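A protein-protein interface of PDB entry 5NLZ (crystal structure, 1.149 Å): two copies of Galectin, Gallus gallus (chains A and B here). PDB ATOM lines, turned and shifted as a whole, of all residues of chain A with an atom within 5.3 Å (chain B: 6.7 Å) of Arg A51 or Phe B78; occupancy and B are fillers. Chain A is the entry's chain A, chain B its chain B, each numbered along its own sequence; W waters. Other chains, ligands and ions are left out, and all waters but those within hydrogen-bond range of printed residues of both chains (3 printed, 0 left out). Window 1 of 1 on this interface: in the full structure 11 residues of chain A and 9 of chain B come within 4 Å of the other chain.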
ATOM      1  N   SER A  30      10.411 -20.560 -17.482  1.00  0.00           N
ATOM      2  CA  SER A  30      10.932 -21.227 -18.668  1.00  0.00           C
ATOM      3  C   SER A  30       9.942 -22.285 -19.138  1.00  0.00           C
ATOM      4  O   SER A  30       8.733 -22.149 -18.913  1.00  0.00           O
ATOM      5  CB  SER A  30      12.337 -21.772 -18.404  1.00  0.00           C
ATOM      6  OG  SER A  30      12.955 -22.208 -19.607  1.00  0.00           O
ATOM      7  N   MET A  31      10.433 -23.343 -19.777  1.00  0.00           N
ATOM      8  CA  MET A  31       9.575 -24.374 -20.334  1.00  0.00           C
ATOM      9  C   MET A  31      10.404 -25.637 -20.509  1.00  0.00           C
ATOM     10  O   MET A  31      11.638 -25.591 -20.518  1.00  0.00           O
ATOM     11  CB  MET A  31       9.008 -23.943 -21.687  1.00  0.00           C
ATOM     12  CG  MET A  31      10.063 -23.729 -22.787  1.00  0.00           C
ATOM     13  SD  MET A  31       9.309 -23.303 -24.368  1.00  0.00           S
ATOM     14  CE  MET A  31       8.639 -21.686 -24.021  1.00  0.00           C
ATOM     15  N   ASN A  49       4.686 -29.807 -24.506  1.00  0.00           N
ATOM     16  CA  ASN A  49       5.486 -28.652 -24.105  1.00  0.00           C
ATOM     17  C   ASN A  49       4.786 -27.785 -23.068  1.00  0.00           C
ATOM     18  O   ASN A  49       4.061 -26.843 -23.419  1.00  0.00           O
ATOM     19  CB  ASN A  49       5.805 -27.870 -25.371  1.00  0.00           C
ATOM     20  CG  ASN A  49       6.555 -26.549 -25.151  1.00  0.00           C
ATOM     21  OD1 ASN A  49       6.343 -25.608 -25.917  1.00  0.00           O
ATOM     22  ND2 ASN A  49       7.401 -26.455 -24.149  1.00  0.00           N
ATOM     23  N   PRO A  50       4.993 -28.067 -21.774  1.00  0.00           N
ATOM     24  CA  PRO A  50       4.527 -27.140 -20.731  1.00  0.00           C
ATOM     25  C   PRO A  50       5.370 -25.874 -20.689  1.00  0.00           C
ATOM     26  O   PRO A  50       6.600 -25.926 -20.572  1.00  0.00           O
ATOM     27  CB  PRO A  50       4.662 -27.957 -19.438  1.00  0.00           C
ATOM     28  CG  PRO A  50       4.711 -29.381 -19.890  1.00  0.00           C
ATOM     29  CD  PRO A  50       5.472 -29.329 -21.188  1.00  0.00           C
ATOM     30  N   ARG A  51       4.686 -24.735 -20.789  1.00  0.00           N
ATOM     31  CA  ARG A  51       5.292 -23.419 -20.956  1.00  0.00           C
ATOM     32  C   ARG A  51       4.907 -22.586 -19.739  1.00  0.00           C
ATOM     33  O   ARG A  51       3.754 -22.157 -19.608  1.00  0.00           O
ATOM     34  CB  ARG A  51       4.811 -22.792 -22.258  1.00  0.00           C
ATOM     35  CG  ARG A  51       5.166 -23.637 -23.480  1.00  0.00           C
ATOM     36  CD  ARG A  51       4.394 -23.266 -24.722  1.00  0.00           C
ATOM     37  NE  ARG A  51       4.757 -21.977 -25.291  1.00  0.00           N
ATOM     38  CZ  ARG A  51       5.751 -21.775 -26.147  1.00  0.00           C
ATOM     39  NH1 ARG A  51       6.517 -22.774 -26.535  1.00  0.00           N
ATOM     40  NH2 ARG A  51       5.973 -20.567 -26.626  1.00  0.00           N
ATOM     41  N   PHE A  52       5.868 -22.371 -18.832  1.00  0.00           N
ATOM     42  CA  PHE A  52       5.561 -21.778 -17.538  1.00  0.00           C
ATOM     43  C   PHE A  52       5.435 -20.264 -17.577  1.00  0.00           C
ATOM     44  O   PHE A  52       4.862 -19.686 -16.654  1.00  0.00           O
ATOM     45  CB  PHE A  52       6.594 -22.218 -16.492  1.00  0.00           C
ATOM     46  CG  PHE A  52       6.435 -23.648 -16.095  1.00  0.00           C
ATOM     47  CD1 PHE A  52       6.878 -24.685 -16.905  1.00  0.00           C
ATOM     48  CD2 PHE A  52       5.772 -23.972 -14.924  1.00  0.00           C
ATOM     49  CE1 PHE A  52       6.677 -26.013 -16.536  1.00  0.00           C
ATOM     50  CE2 PHE A  52       5.579 -25.302 -14.562  1.00  0.00           C
ATOM     51  CZ  PHE A  52       6.025 -26.316 -15.366  1.00  0.00           C
ATOM     52  N   ALA A  53       5.955 -19.595 -18.598  1.00  0.00           N
ATOM     53  CA  ALA A  53       5.785 -18.148 -18.636  1.00  0.00           C
ATOM     54  C   ALA A  53       4.318 -17.781 -18.819  1.00  0.00           C
ATOM     55  O   ALA A  53       3.797 -16.929 -18.101  1.00  0.00           O
ATOM     56  CB  ALA A  53       6.658 -17.509 -19.725  1.00  0.00           C
ATOM     57  N   SER A  54       3.631 -18.429 -19.756  1.00  0.00           N
ATOM     58  CA  SER A  54       2.206 -18.209 -19.968  1.00  0.00           C
ATOM     59  C   SER A  54       1.323 -19.191 -19.212  1.00  0.00           C
ATOM     60  O   SER A  54       0.096 -19.018 -19.188  1.00  0.00           O
ATOM     61  CB  SER A  54       1.860 -18.355 -21.451  1.00  0.00           C
ATOM     62  OG  SER A  54       2.406 -17.308 -22.224  1.00  0.00           O
ATOM     63  N   SER A  55       1.889 -20.248 -18.639  1.00  0.00           N
ATOM     64  CA  SER A  55       1.092 -21.333 -18.060  1.00  0.00           C
ATOM     65  C   SER A  55       0.160 -21.949 -19.100  1.00  0.00           C
ATOM     66  O   SER A  55      -1.051 -22.054 -18.907  1.00  0.00           O
ATOM     67  CB  SER A  55       0.329 -20.878 -16.814  1.00  0.00           C
ATOM     68  OG  SER A  55       1.215 -20.496 -15.768  1.00  0.00           O
ATOM     69  N   ARG A  56       0.749 -22.377 -20.211  1.00  0.00           N
ATOM     70  CA  ARG A  56       0.032 -23.081 -21.263  1.00  0.00           C
ATOM     71  C   ARG A  56       0.810 -24.337 -21.638  1.00  0.00           C
ATOM     72  O   ARG A  56       2.039 -24.347 -21.663  1.00  0.00           O
ATOM     73  CB  ARG A  56      -0.134 -22.196 -22.498  1.00  0.00           C
ATOM     74  CG  ARG A  56      -1.077 -21.021 -22.259  1.00  0.00           C
ATOM     75  CD  ARG A  56      -1.094 -20.043 -23.410  1.00  0.00           C
ATOM     76  NE  ARG A  56      -2.098 -19.011 -23.197  1.00  0.00           N
ATOM     77  CZ  ARG A  56      -2.003 -17.751 -23.594  1.00  0.00           C
ATOM     78  NH1 ARG A  56      -0.920 -17.318 -24.209  1.00  0.00           N
ATOM     79  NH2 ARG A  56      -3.008 -16.919 -23.352  1.00  0.00           N
ATOM     80  N   ILE A  57       0.082 -25.388 -21.977  1.00  0.00           N
ATOM     81  CA  ILE A  57       0.659 -26.580 -22.577  1.00  0.00           C
ATOM     82  C   ILE A  57       0.372 -26.539 -24.063  1.00  0.00           C
ATOM     83  O   ILE A  57      -0.788 -26.405 -24.463  1.00  0.00           O
ATOM     84  CB  ILE A  57       0.075 -27.865 -21.969  1.00  0.00           C
ATOM     85  CG1 ILE A  57       0.360 -27.971 -20.472  1.00  0.00           C
ATOM     86  CG2 ILE A  57       0.622 -29.087 -22.721  1.00  0.00           C
ATOM     87  CD1 ILE A  57      -0.454 -29.032 -19.760  1.00  0.00           C
ATOM     88  N   VAL A  58       1.411 -26.711 -24.874  1.00  0.00           N
ATOM     89  CA  VAL A  58       1.277 -26.849 -26.319  1.00  0.00           C
ATOM     90  C   VAL A  58       1.615 -28.276 -26.689  1.00  0.00           C
ATOM     91  O   VAL A  58       2.641 -28.799 -26.262  1.00  0.00           O
ATOM     92  CB  VAL A  58       2.198 -25.850 -27.054  1.00  0.00           C
ATOM     93  CG1 VAL A  58       2.356 -26.195 -28.542  1.00  0.00           C
ATOM     94  CG2 VAL A  58       1.697 -24.409 -26.856  1.00  0.00           C
ATOM     95  N   PHE A  76      -3.659 -25.766 -16.970  1.00  0.00           N
ATOM     96  CA  PHE A  76      -2.223 -25.882 -16.726  1.00  0.00           C
ATOM     97  C   PHE A  76      -2.047 -26.237 -15.261  1.00  0.00           C
ATOM     98  O   PHE A  76      -1.994 -25.352 -14.404  1.00  0.00           O
ATOM     99  CB  PHE A  76      -1.496 -24.582 -17.061  1.00  0.00           C
ATOM    100  CG  PHE A  76       0.003 -24.696 -17.052  1.00  0.00           C
ATOM    101  CD1 PHE A  76       0.684 -25.116 -18.179  1.00  0.00           C
ATOM    102  CD2 PHE A  76       0.729 -24.369 -15.917  1.00  0.00           C
ATOM    103  CE1 PHE A  76       2.050 -25.194 -18.187  1.00  0.00           C
ATOM    104  CE2 PHE A  76       2.102 -24.455 -15.919  1.00  0.00           C
ATOM    105  CZ  PHE A  76       2.765 -24.861 -17.042  1.00  0.00           C
ATOM    106  N   THR B  25       0.195 -13.246 -33.111  1.00  0.00           N
ATOM    107  CA  THR B  25       1.083 -13.697 -34.165  1.00  0.00           C
ATOM    108  C   THR B  25       0.421 -14.888 -34.831  1.00  0.00           C
ATOM    109  O   THR B  25      -0.117 -15.764 -34.147  1.00  0.00           O
ATOM    110  CB  THR B  25       2.464 -14.031 -33.552  1.00  0.00           C
ATOM    111  OG1 THR B  25       3.085 -12.814 -33.100  1.00  0.00           O
ATOM    112  CG2 THR B  25       3.368 -14.703 -34.547  1.00  0.00           C
ATOM    113  N   PHE B  32       8.313 -11.422 -34.714  1.00  0.00           N
ATOM    114  CA  PHE B  32       8.042 -10.017 -34.955  1.00  0.00           C
ATOM    115  C   PHE B  32       9.072  -9.200 -34.203  1.00  0.00           C
ATOM    116  O   PHE B  32       9.828  -9.727 -33.385  1.00  0.00           O
ATOM    117  CB  PHE B  32       6.604  -9.620 -34.593  1.00  0.00           C
ATOM    118  CG  PHE B  32       6.316  -9.583 -33.115  1.00  0.00           C
ATOM    119  CD1 PHE B  32       5.835 -10.705 -32.456  1.00  0.00           C
ATOM    120  CD2 PHE B  32       6.458  -8.406 -32.395  1.00  0.00           C
ATOM    121  CE1 PHE B  32       5.548 -10.667 -31.098  1.00  0.00           C
ATOM    122  CE2 PHE B  32       6.167  -8.349 -31.028  1.00  0.00           C
ATOM    123  CZ  PHE B  32       5.706  -9.485 -30.385  1.00  0.00           C
ATOM    124  N   PHE B  48      13.590  -5.322 -30.029  1.00  0.00           N
ATOM    125  CA  PHE B  48      12.930  -6.341 -29.218  1.00  0.00           C
ATOM    126  C   PHE B  48      12.304  -7.346 -30.172  1.00  0.00           C
ATOM    127  O   PHE B  48      11.401  -6.985 -30.928  1.00  0.00           O
ATOM    128  CB  PHE B  48      11.862  -5.651 -28.363  1.00  0.00           C
ATOM    129  CG  PHE B  48      10.945  -6.595 -27.627  1.00  0.00           C
ATOM    130  CD1 PHE B  48      11.324  -7.175 -26.422  1.00  0.00           C
ATOM    131  CD2 PHE B  48       9.692  -6.885 -28.129  1.00  0.00           C
ATOM    132  CE1 PHE B  48      10.469  -8.025 -25.747  1.00  0.00           C
ATOM    133  CE2 PHE B  48       8.829  -7.732 -27.449  1.00  0.00           C
ATOM    134  CZ  PHE B  48       9.224  -8.302 -26.259  1.00  0.00           C
ATOM    135  N   PRO B  50      10.784 -11.166 -30.375  1.00  0.00           N
ATOM    136  CA  PRO B  50      10.309 -12.517 -30.015  1.00  0.00           C
ATOM    137  C   PRO B  50      10.349 -13.447 -31.221  1.00  0.00           C
ATOM    138  O   PRO B  50       9.767 -13.152 -32.273  1.00  0.00           O
ATOM    139  CB  PRO B  50       8.872 -12.266 -29.536  1.00  0.00           C
ATOM    140  CG  PRO B  50       8.848 -10.820 -29.139  1.00  0.00           C
ATOM    141  CD  PRO B  50       9.725 -10.159 -30.172  1.00  0.00           C
ATOM    142  N   ARG B  51      11.045 -14.574 -31.047  1.00  0.00           N
ATOM    143  CA  ARG B  51      11.239 -15.585 -32.081  1.00  0.00           C
ATOM    144  C   ARG B  51      10.477 -16.847 -31.668  1.00  0.00           C
ATOM    145  O   ARG B  51      10.882 -17.557 -30.740  1.00  0.00           O
ATOM    146  CB  ARG B  51      12.731 -15.856 -32.264  1.00  0.00           C
ATOM    147  CG  ARG B  51      13.525 -14.621 -32.683  1.00  0.00           C
ATOM    148  CD  ARG B  51      15.005 -14.918 -32.986  1.00  0.00           C
ATOM    149  NE  ARG B  51      15.744 -13.721 -33.415  1.00  0.00           N
ATOM    150  CZ  ARG B  51      17.042 -13.687 -33.720  1.00  0.00           C
ATOM    151  NH1 ARG B  51      17.781 -14.786 -33.664  1.00  0.00           N
ATOM    152  NH2 ARG B  51      17.604 -12.542 -34.090  1.00  0.00           N
ATOM    153  N   PHE B  52       9.347 -17.099 -32.330  1.00  0.00           N
ATOM    154  CA  PHE B  52       8.470 -18.190 -31.916  1.00  0.00           C
ATOM    155  C   PHE B  52       9.045 -19.564 -32.233  1.00  0.00           C
ATOM    156  O   PHE B  52       8.713 -20.534 -31.542  1.00  0.00           O
ATOM    157  CB  PHE B  52       7.082 -18.025 -32.536  1.00  0.00           C
ATOM    158  CG  PHE B  52       6.259 -16.938 -31.902  1.00  0.00           C
ATOM    159  CD1 PHE B  52       6.625 -15.614 -32.026  1.00  0.00           C
ATOM    160  CD2 PHE B  52       5.130 -17.247 -31.172  1.00  0.00           C
ATOM    161  CE1 PHE B  52       5.875 -14.616 -31.433  1.00  0.00           C
ATOM    162  CE2 PHE B  52       4.374 -16.255 -30.575  1.00  0.00           C
ATOM    163  CZ  PHE B  52       4.745 -14.932 -30.712  1.00  0.00           C
ATOM    164  N   SER B  55      11.274 -19.952 -29.228  1.00  0.00           N
ATOM    165  CA  SER B  55      10.755 -19.427 -27.963  1.00  0.00           C
ATOM    166  C   SER B  55      11.840 -18.664 -27.196  1.00  0.00           C
ATOM    167  O   SER B  55      12.089 -18.899 -26.013  1.00  0.00           O
ATOM    168  CB  SER B  55      10.082 -20.511 -27.109  1.00  0.00           C
ATOM    169  OG  SER B  55       8.908 -21.055 -27.732  1.00  0.00           O
ATOM    170  N   ILE B  57      13.393 -14.459 -26.738  1.00  0.00           N
ATOM    171  CA  ILE B  57      13.361 -13.033 -27.051  1.00  0.00           C
ATOM    172  C   ILE B  57      14.795 -12.578 -27.253  1.00  0.00           C
ATOM    173  O   ILE B  57      15.637 -12.761 -26.369  1.00  0.00           O
ATOM    174  CB  ILE B  57      12.699 -12.205 -25.940  1.00  0.00           C
ATOM    175  CG1 ILE B  57      11.280 -12.696 -25.653  1.00  0.00           C
ATOM    176  CG2 ILE B  57      12.702 -10.708 -26.337  1.00  0.00           C
ATOM    177  CD1 ILE B  57      10.620 -12.021 -24.459  1.00  0.00           C
ATOM    178  N   THR B  75      12.651 -16.331 -21.081  1.00  0.00           N
ATOM    179  CA  THR B  75      11.272 -16.112 -20.671  1.00  0.00           C
ATOM    180  C   THR B  75      10.471 -15.693 -21.895  1.00  0.00           C
ATOM    181  O   THR B  75      10.741 -14.642 -22.490  1.00  0.00           O
ATOM    182  CB  THR B  75      11.183 -15.069 -19.569  1.00  0.00           C
ATOM    183  OG1 THR B  75      11.898 -15.551 -18.422  1.00  0.00           O
ATOM    184  CG2 THR B  75       9.739 -14.839 -19.190  1.00  0.00           C
ATOM    185  N   PHE B  76       9.502 -16.520 -22.277  1.00  0.00           N
ATOM    186  CA  PHE B  76       8.809 -16.374 -23.550  1.00  0.00           C
ATOM    187  C   PHE B  76       7.311 -16.507 -23.330  1.00  0.00           C
ATOM    188  O   PHE B  76       6.727 -17.573 -23.563  1.00  0.00           O
ATOM    189  CB  PHE B  76       9.326 -17.396 -24.552  1.00  0.00           C
ATOM    190  CG  PHE B  76       8.965 -17.061 -25.967  1.00  0.00           C
ATOM    191  CD1 PHE B  76       9.703 -16.140 -26.684  1.00  0.00           C
ATOM    192  CD2 PHE B  76       7.868 -17.643 -26.586  1.00  0.00           C
ATOM    193  CE1 PHE B  76       9.360 -15.823 -27.991  1.00  0.00           C
ATOM    194  CE2 PHE B  76       7.529 -17.320 -27.893  1.00  0.00           C
ATOM    195  CZ  PHE B  76       8.280 -16.410 -28.583  1.00  0.00           C
ATOM    196  N   PRO B  77       6.647 -15.426 -22.887  1.00  0.00           N
ATOM    197  CA  PRO B  77       5.215 -15.480 -22.583  1.00  0.00           C
ATOM    198  C   PRO B  77       4.378 -15.187 -23.822  1.00  0.00           C
ATOM    199  O   PRO B  77       3.588 -14.248 -23.861  1.00  0.00           O
ATOM    200  CB  PRO B  77       5.069 -14.402 -21.505  1.00  0.00           C
ATOM    201  CG  PRO B  77       6.140 -13.440 -21.779  1.00  0.00           C
ATOM    202  CD  PRO B  77       7.235 -14.129 -22.518  1.00  0.00           C
ATOM    203  N   PHE B  78       4.567 -16.005 -24.852  1.00  0.00           N
ATOM    204  CA  PHE B  78       3.849 -15.852 -26.105  1.00  0.00           C
ATOM    205  C   PHE B  78       3.523 -17.233 -26.639  1.00  0.00           C
ATOM    206  O   PHE B  78       4.311 -18.168 -26.489  1.00  0.00           O
ATOM    207  CB  PHE B  78       4.686 -15.191 -27.203  1.00  0.00           C
ATOM    208  CG  PHE B  78       5.170 -13.793 -26.908  1.00  0.00           C
ATOM    209  CD1 PHE B  78       4.333 -12.707 -27.089  1.00  0.00           C
ATOM    210  CD2 PHE B  78       6.486 -13.556 -26.525  1.00  0.00           C
ATOM    211  CE1 PHE B  78       4.798 -11.419 -26.877  1.00  0.00           C
ATOM    212  CE2 PHE B  78       6.952 -12.259 -26.304  1.00  0.00           C
ATOM    213  CZ  PHE B  78       6.112 -11.194 -26.491  1.00  0.00           C
ATOM    214  N   GLU B  79       2.378 -17.331 -27.315  1.00  0.00           N
ATOM    215  CA  GLU B  79       1.943 -18.537 -28.005  1.00  0.00           C
ATOM    216  C   GLU B  79       1.265 -18.104 -29.294  1.00  0.00           C
ATOM    217  O   GLU B  79       0.539 -17.100 -29.329  1.00  0.00           O
ATOM    218  CB  GLU B  79       0.980 -19.374 -27.149  1.00  0.00           C
ATOM    219  CG  GLU B  79       1.676 -20.252 -26.123  1.00  0.00           C
ATOM    220  CD  GLU B  79       2.178 -19.512 -24.889  1.00  0.00           C
ATOM    221  OE1 GLU B  79       1.659 -18.416 -24.552  1.00  0.00           O
ATOM    222  OE2 GLU B  79       3.083 -20.086 -24.214  1.00  0.00           O
ATOM    223  N   ALA B  80       1.529 -18.845 -30.364  1.00  0.00           N
ATOM    224  CA  ALA B  80       0.957 -18.501 -31.658  1.00  0.00           C
ATOM    225  C   ALA B  80      -0.553 -18.376 -31.550  1.00  0.00           C
ATOM    226  O   ALA B  80      -1.218 -19.185 -30.893  1.00  0.00           O
ATOM    227  CB  ALA B  80       1.302 -19.570 -32.694  1.00  0.00           C
ATOM    228  N   GLU B  82      -2.424 -16.499 -29.943  1.00  0.00           N
ATOM    229  CA  GLU B  82      -3.009 -16.080 -28.676  1.00  0.00           C
ATOM    230  C   GLU B  82      -2.750 -14.598 -28.479  1.00  0.00           C
ATOM    231  O   GLU B  82      -1.600 -14.163 -28.566  1.00  0.00           O
ATOM    232  CB  GLU B  82      -2.406 -16.855 -27.507  1.00  0.00           C
ATOM    233  CG  GLU B  82      -2.616 -18.360 -27.582  1.00  0.00           C
ATOM    234  CD  GLU B  82      -4.038 -18.809 -27.289  1.00  0.00           C
ATOM    235  OE1 GLU B  82      -4.925 -17.966 -27.027  1.00  0.00           O
ATOM    236  OE2 GLU B  82      -4.272 -20.034 -27.327  1.00  0.00           O
ATOM    237  N   PHE B  84      -1.717 -11.118 -27.009  1.00  0.00           N
ATOM    238  CA  PHE B  84      -0.746 -10.721 -26.005  1.00  0.00           C
ATOM    239  C   PHE B  84      -0.762  -9.203 -25.870  1.00  0.00           C
ATOM    240  O   PHE B  84      -1.293  -8.477 -26.720  1.00  0.00           O
ATOM    241  CB  PHE B  84       0.678 -11.197 -26.337  1.00  0.00           C
ATOM    242  CG  PHE B  84       1.162 -10.787 -27.705  1.00  0.00           C
ATOM    243  CD1 PHE B  84       1.535  -9.479 -27.967  1.00  0.00           C
ATOM    244  CD2 PHE B  84       1.278 -11.726 -28.718  1.00  0.00           C
ATOM    245  CE1 PHE B  84       1.974  -9.114 -29.217  1.00  0.00           C
ATOM    246  CE2 PHE B  84       1.735 -11.369 -29.958  1.00  0.00           C
ATOM    247  CZ  PHE B  84       2.085 -10.057 -30.213  1.00  0.00           C
ATOM    248  N   GLN B  85      -0.135  -8.736 -24.798  1.00  0.00           N
ATOM    249  CA  GLN B  85       0.045  -7.316 -24.532  1.00  0.00           C
ATOM    250  C   GLN B  85       1.482  -7.112 -24.092  1.00  0.00           C
ATOM    251  O   GLN B  85       1.898  -7.660 -23.072  1.00  0.00           O
ATOM    252  CB  GLN B  85      -0.903  -6.859 -23.426  1.00  0.00           C
ATOM    253  CG  GLN B  85      -0.731  -5.416 -23.032  1.00  0.00           C
ATOM    254  CD  GLN B  85      -1.704  -5.007 -21.967  1.00  0.00           C
ATOM    255  OE1 GLN B  85      -2.913  -5.216 -22.108  1.00  0.00           O
ATOM    256  NE2 GLN B  85      -1.190  -4.441 -20.875  1.00  0.00           N
ATOM    257  N   VAL B  86       2.227  -6.302 -24.837  1.00  0.00           N
ATOM    258  CA  VAL B  86       3.612  -5.965 -24.521  1.00  0.00           C
ATOM    259  C   VAL B  86       3.645  -4.505 -24.110  1.00  0.00           C
ATOM    260  O   VAL B  86       3.205  -3.639 -24.872  1.00  0.00           O
ATOM    261  CB  VAL B  86       4.533  -6.187 -25.725  1.00  0.00           C
ATOM    262  CG1 VAL B  86       5.966  -5.791 -25.397  1.00  0.00           C
ATOM    263  CG2 VAL B  86       4.477  -7.630 -26.163  1.00  0.00           C
ATOM    264  N   ILE B  97      10.446  -4.233 -20.008  1.00  0.00           N
ATOM    265  CA  ILE B  97       9.437  -4.977 -20.766  1.00  0.00           C
ATOM    266  C   ILE B  97       8.550  -5.709 -19.772  1.00  0.00           C
ATOM    267  O   ILE B  97       9.044  -6.503 -18.966  1.00  0.00           O
ATOM    268  CB  ILE B  97      10.070  -6.017 -21.708  1.00  0.00           C
ATOM    269  CG1 ILE B  97      11.013  -5.381 -22.740  1.00  0.00           C
ATOM    270  CG2 ILE B  97       8.975  -6.850 -22.401  1.00  0.00           C
ATOM    271  CD1 ILE B  97      10.335  -4.587 -23.784  1.00  0.00           C
ATOM    272  N   ILE B  99       5.047  -8.133 -19.957  1.00  0.00           N
ATOM    273  CA  ILE B  99       4.201  -8.864 -20.893  1.00  0.00           C
ATOM    274  C   ILE B  99       3.099  -9.528 -20.112  1.00  0.00           C
ATOM    275  O   ILE B  99       3.362 -10.169 -19.088  1.00  0.00           O
ATOM    276  CB  ILE B  99       4.969  -9.897 -21.733  1.00  0.00           C
ATOM    277  CG1 ILE B  99       6.018  -9.177 -22.587  1.00  0.00           C
ATOM    278  CG2 ILE B  99       3.995 -10.678 -22.630  1.00  0.00           C
ATOM    279  CD1 ILE B  99       6.958 -10.093 -23.315  1.00  0.00           C
ATOM    280  N   ASP B 100       1.872  -9.362 -20.593  1.00  0.00           N
ATOM    281  CA  ASP B 100       0.679  -9.853 -19.928  1.00  0.00           C
ATOM    282  C   ASP B 100       0.792  -9.489 -18.442  1.00  0.00           C
ATOM    283  O   ASP B 100       0.489 -10.288 -17.552  1.00  0.00           O
ATOM    284  CB  ASP B 100       0.449 -11.342 -20.279  1.00  0.00           C
ATOM    285  CG  ASP B 100       0.314 -11.603 -21.841  1.00  0.00           C
ATOM    286  OD1 ASP B 100       0.013 -10.657 -22.627  1.00  0.00           O
ATOM    287  OD2 ASP B 100       0.507 -12.775 -22.288  1.00  0.00           O
HETATM  288  O   HOH W   1       4.971 -19.284 -22.394  1.00  0.00           O
HETATM  289  O   HOH W   2      -0.661 -14.467 -24.682  1.00  0.00           O
HETATM  290  O   HOH W   3       1.175 -15.109 -21.192  1.00  0.00           O
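Water W3 lies within hydrogen-bond range of the side-chain carboxylate (OD2) of Asp B100 (2.7 Å) and the side-chain hydroxyl (OG) of Ser A54 (2.7 Å). Water W1 lies within hydrogen-bond range of O of Phe B76 (2.7 Å), OE2 of Glu B79 (2.7 Å) and N of Ser A54 (3.1 Å). Water W2 bridges the guanidinium group (NH1) of Arg A56 and the side-chain carboxylate (OD2) of Asp B100.
ND2 of Asn A49 is in hydrogen-bond range of SD of Met A31, at 3.7 Å. The guanidinium group (NH1) of Arg A51 sits close to the side-chain sulfur (SD) of Met A31 (3.6 Å). OD1 of Asn A49 sits at hydrogen-bond distance from NH1 of Arg A51. The backbone NH (N) of Arg A51 lies within hydrogen-bond range of the backbone carbonyl oxygen (O) of Arg A56 (2.8 Å).
Met A31 touches Ser B55. CD2 of Phe B76 touches NH2 of Arg A51 (3.5 Å). Ala A53 touches Phe B76. Ala A53 touches Pro B77 (CB to N, 3.8 Å). OG of Ser A54 touches C of Pro B77 (3.3 Å). Phe B78 touches Ser A54 (N to OG, 3.6 Å). NH1 of Arg A56 touches CB of Glu B82, at 3.6 Å.
Printed residues of chain B that touch a printed residue of chain A: Ser B55, Phe B76, Pro B77, Phe B78, Glu B79 and Glu B82. Hydrophobic or aromatic side chains of chain B within 4 Å of the printed part of chain A: Phe B76 and Pro B77. Hydrophobic or aromatic side chains of chain A within 4 Å of the printed part of chain B: Met A31 and Ala A53. Among the printed residues, 12 pairs touch across the chains.
NH2 of Arg A51 sits at hydrogen-bond distance from OG of Ser B55, at 3.2 Å. The guanidinium group (NH2) of Arg A51 sits at hydrogen-bond distance from the backbone carbonyl oxygen (O) of Phe B78 (2.9 Å). The side-chain carboxylate (OE2) of Glu B79 is in salt-bridge range of the guanidinium group (NE) of Arg A51 (2.7 Å). The side-chain hydroxyl (OG) of Ser A54 is in hydrogen-bond range of the side-chain carboxylate (OE1) of Glu B79 (2.7 Å). NH1 of Arg A56 lies within salt-bridge range of OE1 of Glu B79 (2.8 Å).
Of chain B, only Ser B55, Phe B76, Phe B78 and Glu B79 come within 4 Å of Arg A51. Phe B78 touches two residues of chain A. Of the printed residues of chain B, Met A31 touches Ser B55 (3.6 Å). Of the printed residues of chain B, Ser A54 touches Pro B77, Phe B78 and Glu B79. Printed residues of chain A within 4 Å of Glu B79: Arg A51 (2.7 Å), Ser A54 (2.7 Å) and Arg A56 (2.8 Å).
Arg A51 touches Ser B55, but with the chains exchanged Ser A55 does not touch Arg B51 (15.3 Å). Arg A51 touches Phe B76, but with the chains exchanged Phe A76 does not touch Arg B51 (17.1 Å). Positions printed for both chains: 50, 51, 52, 55, 57 and 76.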
